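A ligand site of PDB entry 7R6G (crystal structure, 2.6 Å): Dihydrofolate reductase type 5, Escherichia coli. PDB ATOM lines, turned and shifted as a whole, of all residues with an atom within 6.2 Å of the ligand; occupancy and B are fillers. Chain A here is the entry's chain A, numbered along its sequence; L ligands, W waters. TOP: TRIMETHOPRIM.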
ATOM      1  N   MET A   6     -23.173 -24.164  16.424  1.00  0.00           N
ATOM      2  CA  MET A   6     -23.222 -25.456  15.702  1.00  0.00           C
ATOM      3  C   MET A   6     -24.243 -25.392  14.555  1.00  0.00           C
ATOM      4  O   MET A   6     -25.402 -25.120  14.782  1.00  0.00           O
ATOM      5  CB  MET A   6     -23.486 -26.628  16.651  1.00  0.00           C
ATOM      6  CG  MET A   6     -23.511 -27.959  15.925  1.00  0.00           C
ATOM      7  SD  MET A   6     -22.743 -29.383  16.745  1.00  0.00           S
ATOM      8  CE  MET A   6     -23.028 -28.890  18.442  1.00  0.00           C
ATOM      9  N   ALA A   7     -23.807 -25.691  13.345  1.00  0.00           N
ATOM     10  CA  ALA A   7     -24.639 -25.638  12.137  1.00  0.00           C
ATOM     11  C   ALA A   7     -24.250 -26.679  11.127  1.00  0.00           C
ATOM     12  O   ALA A   7     -23.097 -27.167  11.120  1.00  0.00           O
ATOM     13  CB  ALA A   7     -24.471 -24.298  11.500  1.00  0.00           C
ATOM     14  N   ALA A   8     -25.194 -26.921  10.232  1.00  0.00           N
ATOM     15  CA  ALA A   8     -25.046 -27.834   9.094  1.00  0.00           C
ATOM     16  C   ALA A   8     -25.600 -27.101   7.887  1.00  0.00           C
ATOM     17  O   ALA A   8     -26.772 -26.704   7.935  1.00  0.00           O
ATOM     18  CB  ALA A   8     -25.747 -29.169   9.366  1.00  0.00           C
ATOM     19  N   ILE A  21     -35.289 -28.825   6.432  1.00  0.00           N
ATOM     20  CA  ILE A  21     -33.906 -28.929   5.906  1.00  0.00           C
ATOM     21  C   ILE A  21     -33.989 -29.764   4.622  1.00  0.00           C
ATOM     22  O   ILE A  21     -34.334 -30.958   4.674  1.00  0.00           O
ATOM     23  CB  ILE A  21     -32.977 -29.536   6.997  1.00  0.00           C
ATOM     24  CG1 ILE A  21     -32.779 -28.583   8.170  1.00  0.00           C
ATOM     25  CG2 ILE A  21     -31.633 -30.011   6.431  1.00  0.00           C
ATOM     26  CD1 ILE A  21     -32.344 -29.301   9.438  1.00  0.00           C
ATOM     27  N   GLU A  28     -24.631 -37.404   9.913  1.00  0.00           N
ATOM     28  CA  GLU A  28     -24.192 -36.019  10.253  1.00  0.00           C
ATOM     29  C   GLU A  28     -24.734 -35.653  11.630  1.00  0.00           C
ATOM     30  O   GLU A  28     -23.960 -35.132  12.470  1.00  0.00           O
ATOM     31  CB  GLU A  28     -24.591 -35.016   9.159  1.00  0.00           C
ATOM     32  CG  GLU A  28     -23.974 -33.642   9.288  1.00  0.00           C
ATOM     33  CD  GLU A  28     -24.499 -32.811  10.463  1.00  0.00           C
ATOM     34  OE1 GLU A  28     -25.752 -32.875  10.715  1.00  0.00           O
ATOM     35  OE2 GLU A  28     -23.649 -32.132  11.151  1.00  0.00           O
ATOM     36  N   GLN A  29     -26.008 -35.979  11.887  1.00  0.00           N
ATOM     37  CA  GLN A  29     -26.703 -35.446  13.080  1.00  0.00           C
ATOM     38  C   GLN A  29     -26.100 -36.089  14.327  1.00  0.00           C
ATOM     39  O   GLN A  29     -26.287 -35.497  15.392  1.00  0.00           O
ATOM     40  CB  GLN A  29     -28.233 -35.590  12.989  1.00  0.00           C
ATOM     41  CG  GLN A  29     -28.783 -36.942  13.450  1.00  0.00           C
ATOM     42  CD  GLN A  29     -30.292 -37.005  13.539  1.00  0.00           C
ATOM     43  OE1 GLN A  29     -30.978 -36.584  12.629  1.00  0.00           O
ATOM     44  NE2 GLN A  29     -30.829 -37.633  14.568  1.00  0.00           N
ATOM     45  N   LEU A  31     -23.173 -35.792  15.204  1.00  0.00           N
ATOM     46  CA  LEU A  31     -22.183 -34.798  15.678  1.00  0.00           C
ATOM     47  C   LEU A  31     -22.952 -33.766  16.498  1.00  0.00           C
ATOM     48  O   LEU A  31     -22.532 -33.422  17.587  1.00  0.00           O
ATOM     49  CB  LEU A  31     -21.453 -34.169  14.481  1.00  0.00           C
ATOM     50  CG  LEU A  31     -20.519 -35.113  13.709  1.00  0.00           C
ATOM     51  CD1 LEU A  31     -20.314 -34.656  12.275  1.00  0.00           C
ATOM     52  CD2 LEU A  31     -19.165 -35.254  14.392  1.00  0.00           C
ATOM     53  N   PHE A  32     -24.076 -33.317  15.996  1.00  0.00           N
ATOM     54  CA  PHE A  32     -24.989 -32.408  16.727  1.00  0.00           C
ATOM     55  C   PHE A  32     -25.362 -33.089  18.050  1.00  0.00           C
ATOM     56  O   PHE A  32     -25.267 -32.380  19.082  1.00  0.00           O
ATOM     57  CB  PHE A  32     -26.217 -32.020  15.900  1.00  0.00           C
ATOM     58  CG  PHE A  32     -27.164 -31.097  16.650  1.00  0.00           C
ATOM     59  CD1 PHE A  32     -26.925 -29.735  16.729  1.00  0.00           C
ATOM     60  CD2 PHE A  32     -28.231 -31.597  17.350  1.00  0.00           C
ATOM     61  CE1 PHE A  32     -27.779 -28.894  17.410  1.00  0.00           C
ATOM     62  CE2 PHE A  32     -29.074 -30.763  18.062  1.00  0.00           C
ATOM     63  CZ  PHE A  32     -28.851 -29.404  18.078  1.00  0.00           C
ATOM     64  N   LYS A  33     -25.766 -34.376  18.052  1.00  0.00           N
ATOM     65  CA  LYS A  33     -26.265 -35.038  19.272  1.00  0.00           C
ATOM     66  C   LYS A  33     -25.103 -35.142  20.252  1.00  0.00           C
ATOM     67  O   LYS A  33     -25.272 -34.800  21.423  1.00  0.00           O
ATOM     68  CB  LYS A  33     -26.881 -36.405  18.989  1.00  0.00           C
ATOM     69  CG  LYS A  33     -28.062 -36.407  18.024  1.00  0.00           C
ATOM     70  CD  LYS A  33     -29.413 -35.931  18.567  1.00  0.00           C
ATOM     71  CE  LYS A  33     -30.237 -37.031  19.221  1.00  0.00           C
ATOM     72  NZ  LYS A  33     -31.271 -37.528  18.296  1.00  0.00           N
ATOM     73  N   LEU A  41     -28.467 -24.838  24.869  1.00  0.00           N
ATOM     74  CA  LEU A  41     -28.516 -24.391  23.463  1.00  0.00           C
ATOM     75  C   LEU A  41     -29.354 -23.119  23.400  1.00  0.00           C
ATOM     76  O   LEU A  41     -30.373 -23.030  24.107  1.00  0.00           O
ATOM     77  CB  LEU A  41     -29.113 -25.422  22.517  1.00  0.00           C
ATOM     78  CG  LEU A  41     -28.836 -26.890  22.834  1.00  0.00           C
ATOM     79  CD1 LEU A  41     -29.483 -27.746  21.773  1.00  0.00           C
ATOM     80  CD2 LEU A  41     -27.361 -27.189  22.938  1.00  0.00           C
ATOM     81  N   VAL A  43     -31.552 -21.108  20.738  1.00  0.00           N
ATOM     82  CA  VAL A  43     -32.294 -21.259  19.453  1.00  0.00           C
ATOM     83  C   VAL A  43     -33.316 -20.116  19.351  1.00  0.00           C
ATOM     84  O   VAL A  43     -33.909 -19.733  20.372  1.00  0.00           O
ATOM     85  CB  VAL A  43     -33.014 -22.595  19.364  1.00  0.00           C
ATOM     86  CG1 VAL A  43     -32.077 -23.737  19.078  1.00  0.00           C
ATOM     87  CG2 VAL A  43     -33.738 -22.847  20.641  1.00  0.00           C
ATOM     88  N   THR A  47     -37.021 -21.893  14.850  1.00  0.00           N
ATOM     89  CA  THR A  47     -36.241 -23.146  14.765  1.00  0.00           C
ATOM     90  C   THR A  47     -36.742 -24.062  15.870  1.00  0.00           C
ATOM     91  O   THR A  47     -36.828 -25.291  15.639  1.00  0.00           O
ATOM     92  CB  THR A  47     -34.725 -22.872  14.796  1.00  0.00           C
ATOM     93  OG1 THR A  47     -34.295 -22.436  13.499  1.00  0.00           O
ATOM     94  CG2 THR A  47     -33.897 -24.075  15.193  1.00  0.00           C
ATOM     95  N   MET A  51     -38.268 -27.690  15.032  1.00  0.00           N
ATOM     96  CA  MET A  51     -37.324 -28.833  15.200  1.00  0.00           C
ATOM     97  C   MET A  51     -37.554 -29.528  16.548  1.00  0.00           C
ATOM     98  O   MET A  51     -37.050 -30.647  16.678  1.00  0.00           O
ATOM     99  CB  MET A  51     -35.858 -28.383  15.116  1.00  0.00           C
ATOM    100  CG  MET A  51     -35.560 -27.686  13.812  1.00  0.00           C
ATOM    101  SD  MET A  51     -34.606 -28.562  12.593  1.00  0.00           S
ATOM    102  CE  MET A  51     -34.259 -30.156  13.324  1.00  0.00           C
ATOM    103  N   GLY A  52     -38.238 -28.887  17.504  1.00  0.00           N
ATOM    104  CA  GLY A  52     -38.634 -29.519  18.767  1.00  0.00           C
ATOM    105  C   GLY A  52     -37.484 -29.666  19.749  1.00  0.00           C
ATOM    106  O   GLY A  52     -36.338 -29.791  19.318  1.00  0.00           O
ATOM    107  N   ALA A  53     -37.791 -29.593  21.041  1.00  0.00           N
ATOM    108  CA  ALA A  53     -36.871 -29.891  22.154  1.00  0.00           C
ATOM    109  C   ALA A  53     -36.394 -31.341  21.982  1.00  0.00           C
ATOM    110  O   ALA A  53     -37.195 -32.191  21.500  1.00  0.00           O
ATOM    111  CB  ALA A  53     -37.574 -29.684  23.466  1.00  0.00           C
ATOM    112  N   LEU A  54     -35.119 -31.611  22.283  1.00  0.00           N
ATOM    113  CA  LEU A  54     -34.596 -32.970  22.454  1.00  0.00           C
ATOM    114  C   LEU A  54     -34.539 -33.245  23.949  1.00  0.00           C
ATOM    115  O   LEU A  54     -34.398 -32.348  24.770  1.00  0.00           O
ATOM    116  CB  LEU A  54     -33.187 -33.102  21.859  1.00  0.00           C
ATOM    117  CG  LEU A  54     -33.109 -33.153  20.334  1.00  0.00           C
ATOM    118  CD1 LEU A  54     -31.648 -32.990  19.896  1.00  0.00           C
ATOM    119  CD2 LEU A  54     -33.709 -34.449  19.767  1.00  0.00           C
ATOM    120  N   TYR A  59     -32.630 -25.458  26.995  1.00  0.00           N
ATOM    121  CA  TYR A  59     -32.926 -24.491  25.920  1.00  0.00           C
ATOM    122  C   TYR A  59     -33.177 -23.098  26.487  1.00  0.00           C
ATOM    123  O   TYR A  59     -33.977 -22.949  27.357  1.00  0.00           O
ATOM    124  CB  TYR A  59     -34.129 -24.965  25.123  1.00  0.00           C
ATOM    125  CG  TYR A  59     -33.840 -26.211  24.332  1.00  0.00           C
ATOM    126  CD1 TYR A  59     -34.033 -27.465  24.882  1.00  0.00           C
ATOM    127  CD2 TYR A  59     -33.402 -26.126  23.024  1.00  0.00           C
ATOM    128  CE1 TYR A  59     -33.766 -28.610  24.156  1.00  0.00           C
ATOM    129  CE2 TYR A  59     -33.105 -27.251  22.294  1.00  0.00           C
ATOM    130  CZ  TYR A  59     -33.301 -28.508  22.858  1.00  0.00           C
ATOM    131  OH  TYR A  59     -33.051 -29.617  22.100  1.00  0.00           O
ATOM    132  N   VAL A  96     -24.985 -22.015  20.463  1.00  0.00           N
ATOM    133  CA  VAL A  96     -25.984 -21.414  19.542  1.00  0.00           C
ATOM    134  C   VAL A  96     -26.280 -22.456  18.476  1.00  0.00           C
ATOM    135  O   VAL A  96     -25.347 -22.868  17.813  1.00  0.00           O
ATOM    136  CB  VAL A  96     -25.437 -20.113  18.926  1.00  0.00           C
ATOM    137  CG1 VAL A  96     -26.417 -19.539  17.943  1.00  0.00           C
ATOM    138  CG2 VAL A  96     -25.100 -19.109  20.021  1.00  0.00           C
ATOM    139  N   SER A  97     -27.524 -22.890  18.371  1.00  0.00           N
ATOM    140  CA  SER A  97     -27.946 -24.010  17.497  1.00  0.00           C
ATOM    141  C   SER A  97     -28.989 -23.546  16.482  1.00  0.00           C
ATOM    142  O   SER A  97     -29.694 -24.366  15.989  1.00  0.00           O
ATOM    143  CB  SER A  97     -28.467 -25.112  18.368  1.00  0.00           C
ATOM    144  OG  SER A  97     -27.461 -25.497  19.299  1.00  0.00           O
ATOM    145  N   GLY A  98     -29.067 -22.249  16.215  1.00  0.00           N
ATOM    146  CA  GLY A  98     -29.668 -21.782  14.970  1.00  0.00           C
ATOM    147  C   GLY A  98     -31.019 -21.090  15.069  1.00  0.00           C
ATOM    148  O   GLY A  98     -31.524 -20.773  16.181  1.00  0.00           O
ATOM    149  N   TYR A 103     -27.976 -16.946  13.935  1.00  0.00           N
ATOM    150  CA  TYR A 103     -26.584 -17.245  13.548  1.00  0.00           C
ATOM    151  C   TYR A 103     -25.938 -15.909  13.199  1.00  0.00           C
ATOM    152  O   TYR A 103     -24.805 -15.608  13.716  1.00  0.00           O
ATOM    153  CB  TYR A 103     -26.549 -18.255  12.393  1.00  0.00           C
ATOM    154  CG  TYR A 103     -26.731 -19.724  12.736  1.00  0.00           C
ATOM    155  CD1 TYR A 103     -26.228 -20.294  13.892  1.00  0.00           C
ATOM    156  CD2 TYR A 103     -27.345 -20.573  11.832  1.00  0.00           C
ATOM    157  CE1 TYR A 103     -26.347 -21.646  14.143  1.00  0.00           C
ATOM    158  CE2 TYR A 103     -27.503 -21.933  12.073  1.00  0.00           C
ATOM    159  CZ  TYR A 103     -26.986 -22.470  13.217  1.00  0.00           C
ATOM    160  OH  TYR A 103     -27.103 -23.812  13.375  1.00  0.00           O
ATOM    161  N   HIS A 114     -18.771 -25.091  15.123  1.00  0.00           N
ATOM    162  CA  HIS A 114     -18.855 -26.509  14.697  1.00  0.00           C
ATOM    163  C   HIS A 114     -19.661 -26.513  13.398  1.00  0.00           C
ATOM    164  O   HIS A 114     -20.887 -26.312  13.497  1.00  0.00           O
ATOM    165  CB  HIS A 114     -19.488 -27.344  15.780  1.00  0.00           C
ATOM    166  CG  HIS A 114     -18.718 -27.398  17.028  1.00  0.00           C
ATOM    167  ND1 HIS A 114     -17.790 -28.394  17.266  1.00  0.00           N
ATOM    168  CD2 HIS A 114     -18.828 -26.684  18.169  1.00  0.00           C
ATOM    169  CE1 HIS A 114     -17.308 -28.269  18.499  1.00  0.00           C
ATOM    170  NE2 HIS A 114     -17.952 -27.215  19.082  1.00  0.00           N
ATOM    171  N   ILE A 115     -18.990 -26.616  12.261  1.00  0.00           N
ATOM    172  CA  ILE A 115     -19.671 -26.469  10.943  1.00  0.00           C
ATOM    173  C   ILE A 115     -19.633 -27.773  10.169  1.00  0.00           C
ATOM    174  O   ILE A 115     -18.525 -28.291   9.923  1.00  0.00           O
ATOM    175  CB  ILE A 115     -19.039 -25.348  10.130  1.00  0.00           C
ATOM    176  CG1 ILE A 115     -18.966 -24.054  10.939  1.00  0.00           C
ATOM    177  CG2 ILE A 115     -19.812 -25.148   8.829  1.00  0.00           C
ATOM    178  CD1 ILE A 115     -20.324 -23.497  11.277  1.00  0.00           C
ATOM    179  N   SER A 116     -20.805 -28.279   9.801  1.00  0.00           N
ATOM    180  CA  SER A 116     -20.962 -29.426   8.878  1.00  0.00           C
ATOM    181  C   SER A 116     -21.406 -28.894   7.525  1.00  0.00           C
ATOM    182  O   SER A 116     -22.366 -28.089   7.486  1.00  0.00           O
ATOM    183  CB  SER A 116     -21.900 -30.422   9.416  1.00  0.00           C
ATOM    184  OG  SER A 116     -21.318 -31.042  10.538  1.00  0.00           O
HETATM  185  C1  TOP L   1     -27.707 -30.252  12.311  1.00  0.00           C
HETATM  186  N2  TOP L   1     -26.405 -30.572  12.368  1.00  0.00           N
HETATM  187  C3  TOP L   1     -25.598 -29.703  13.019  1.00  0.00           C
HETATM  188  N4  TOP L   1     -24.305 -29.996  13.118  1.00  0.00           N
HETATM  189  N5  TOP L   1     -26.024 -28.564  13.600  1.00  0.00           N
HETATM  190  C6  TOP L   1     -27.334 -28.256  13.524  1.00  0.00           C
HETATM  191  N7  TOP L   1     -27.730 -27.097  14.101  1.00  0.00           N
HETATM  192  C8  TOP L   1     -28.237 -29.092  12.847  1.00  0.00           C
HETATM  193  C9  TOP L   1     -29.722 -28.792  12.793  1.00  0.00           C
HETATM  194  C10 TOP L   1     -30.469 -29.422  13.956  1.00  0.00           C
HETATM  195  C11 TOP L   1     -30.956 -28.645  15.007  1.00  0.00           C
HETATM  196  C12 TOP L   1     -31.633 -29.224  16.078  1.00  0.00           C
HETATM  197  O13 TOP L   1     -32.145 -28.523  17.143  1.00  0.00           O
HETATM  198  C14 TOP L   1     -31.909 -27.117  17.143  1.00  0.00           C
HETATM  199  C15 TOP L   1     -31.785 -30.627  16.125  1.00  0.00           C
HETATM  200  O16 TOP L   1     -32.441 -31.255  17.159  1.00  0.00           O
HETATM  201  C17 TOP L   1     -33.860 -31.123  17.143  1.00  0.00           C
HETATM  202  C18 TOP L   1     -31.298 -31.418  15.078  1.00  0.00           C
HETATM  203  O19 TOP L   1     -31.539 -32.755  15.234  1.00  0.00           O
HETATM  204  C20 TOP L   1     -30.674 -33.694  14.598  1.00  0.00           C
HETATM  205  C21 TOP L   1     -30.657 -30.815  14.005  1.00  0.00           C
HETATM  206  O   HOH W   1     -21.297 -28.990  13.230  1.00  0.00           O
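CA of Ala 7 touches N5 of the ligand, 3.6 Å away. Ala 8 touches the ligand (CB to N2, 3.4 Å). Gln 29 touches the ligand. CE2 of Phe 32 touches C15 of the ligand, 3.3 Å away. Val 43 touches the ligand (CG1 to C14, 3.9 Å). Met 51 touches the ligand (O to C17, 3.3 Å). Gly 52 touches the ligand. Leu 54 touches the ligand. Ser 97 touches the ligand. 12 residues have an atom within 4 Å of the ligand: Met 6, Ala 7, Ala 8, Glu 28, Gln 29, Phe 32, Val 43, Met 51, Gly 52, Leu 54, Ser 97 and Tyr 103.
The side-chain carboxylate (OE2) of Glu 28 lies within hydrogen-bond range of the side-chain hydroxyl (OG) of Ser 116. The backbone carbonyl oxygen (O) of Met 6 is in hydrogen-bond range of the side-chain hydroxyl (OH) of Tyr 103. O of Val 96 is in hydrogen-bond range of N of Met 6, 2.9 Å away. The backbone NH (N) of Leu 54 sits at hydrogen-bond distance from the side-chain hydroxyl (OH) of Tyr 59. The backbone NH (N) of Ser 116 sits at hydrogen-bond distance from the backbone carbonyl oxygen (O) of Ala 7 (2.9 Å). N of Ala 7 sits at hydrogen-bond distance from O of His 114, at 3.0 Å.
Water W1 lies within hydrogen-bond range of the backbone carbonyl oxygen of His 114 (2.7 Å), a nitrogen (N4) of the ligand (3.2 Å), the backbone carbonyl oxygen of Ala 7 (3.3 Å), the side-chain hydroxyl of Ser 116 (3.4 Å) and the backbone NH of Ile 115 (3.4 Å).
A nitrogen (N4) of the ligand sits at hydrogen-bond distance from the side-chain carboxylate (OE2) of Glu 28. N7 of the ligand sits at hydrogen-bond distance from O of Met 6, at 3.1 Å. The side-chain hydroxyl (OH) of Tyr 103 sits at hydrogen-bond distance from a nitrogen (N7) of the ligand (3.4 Å).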
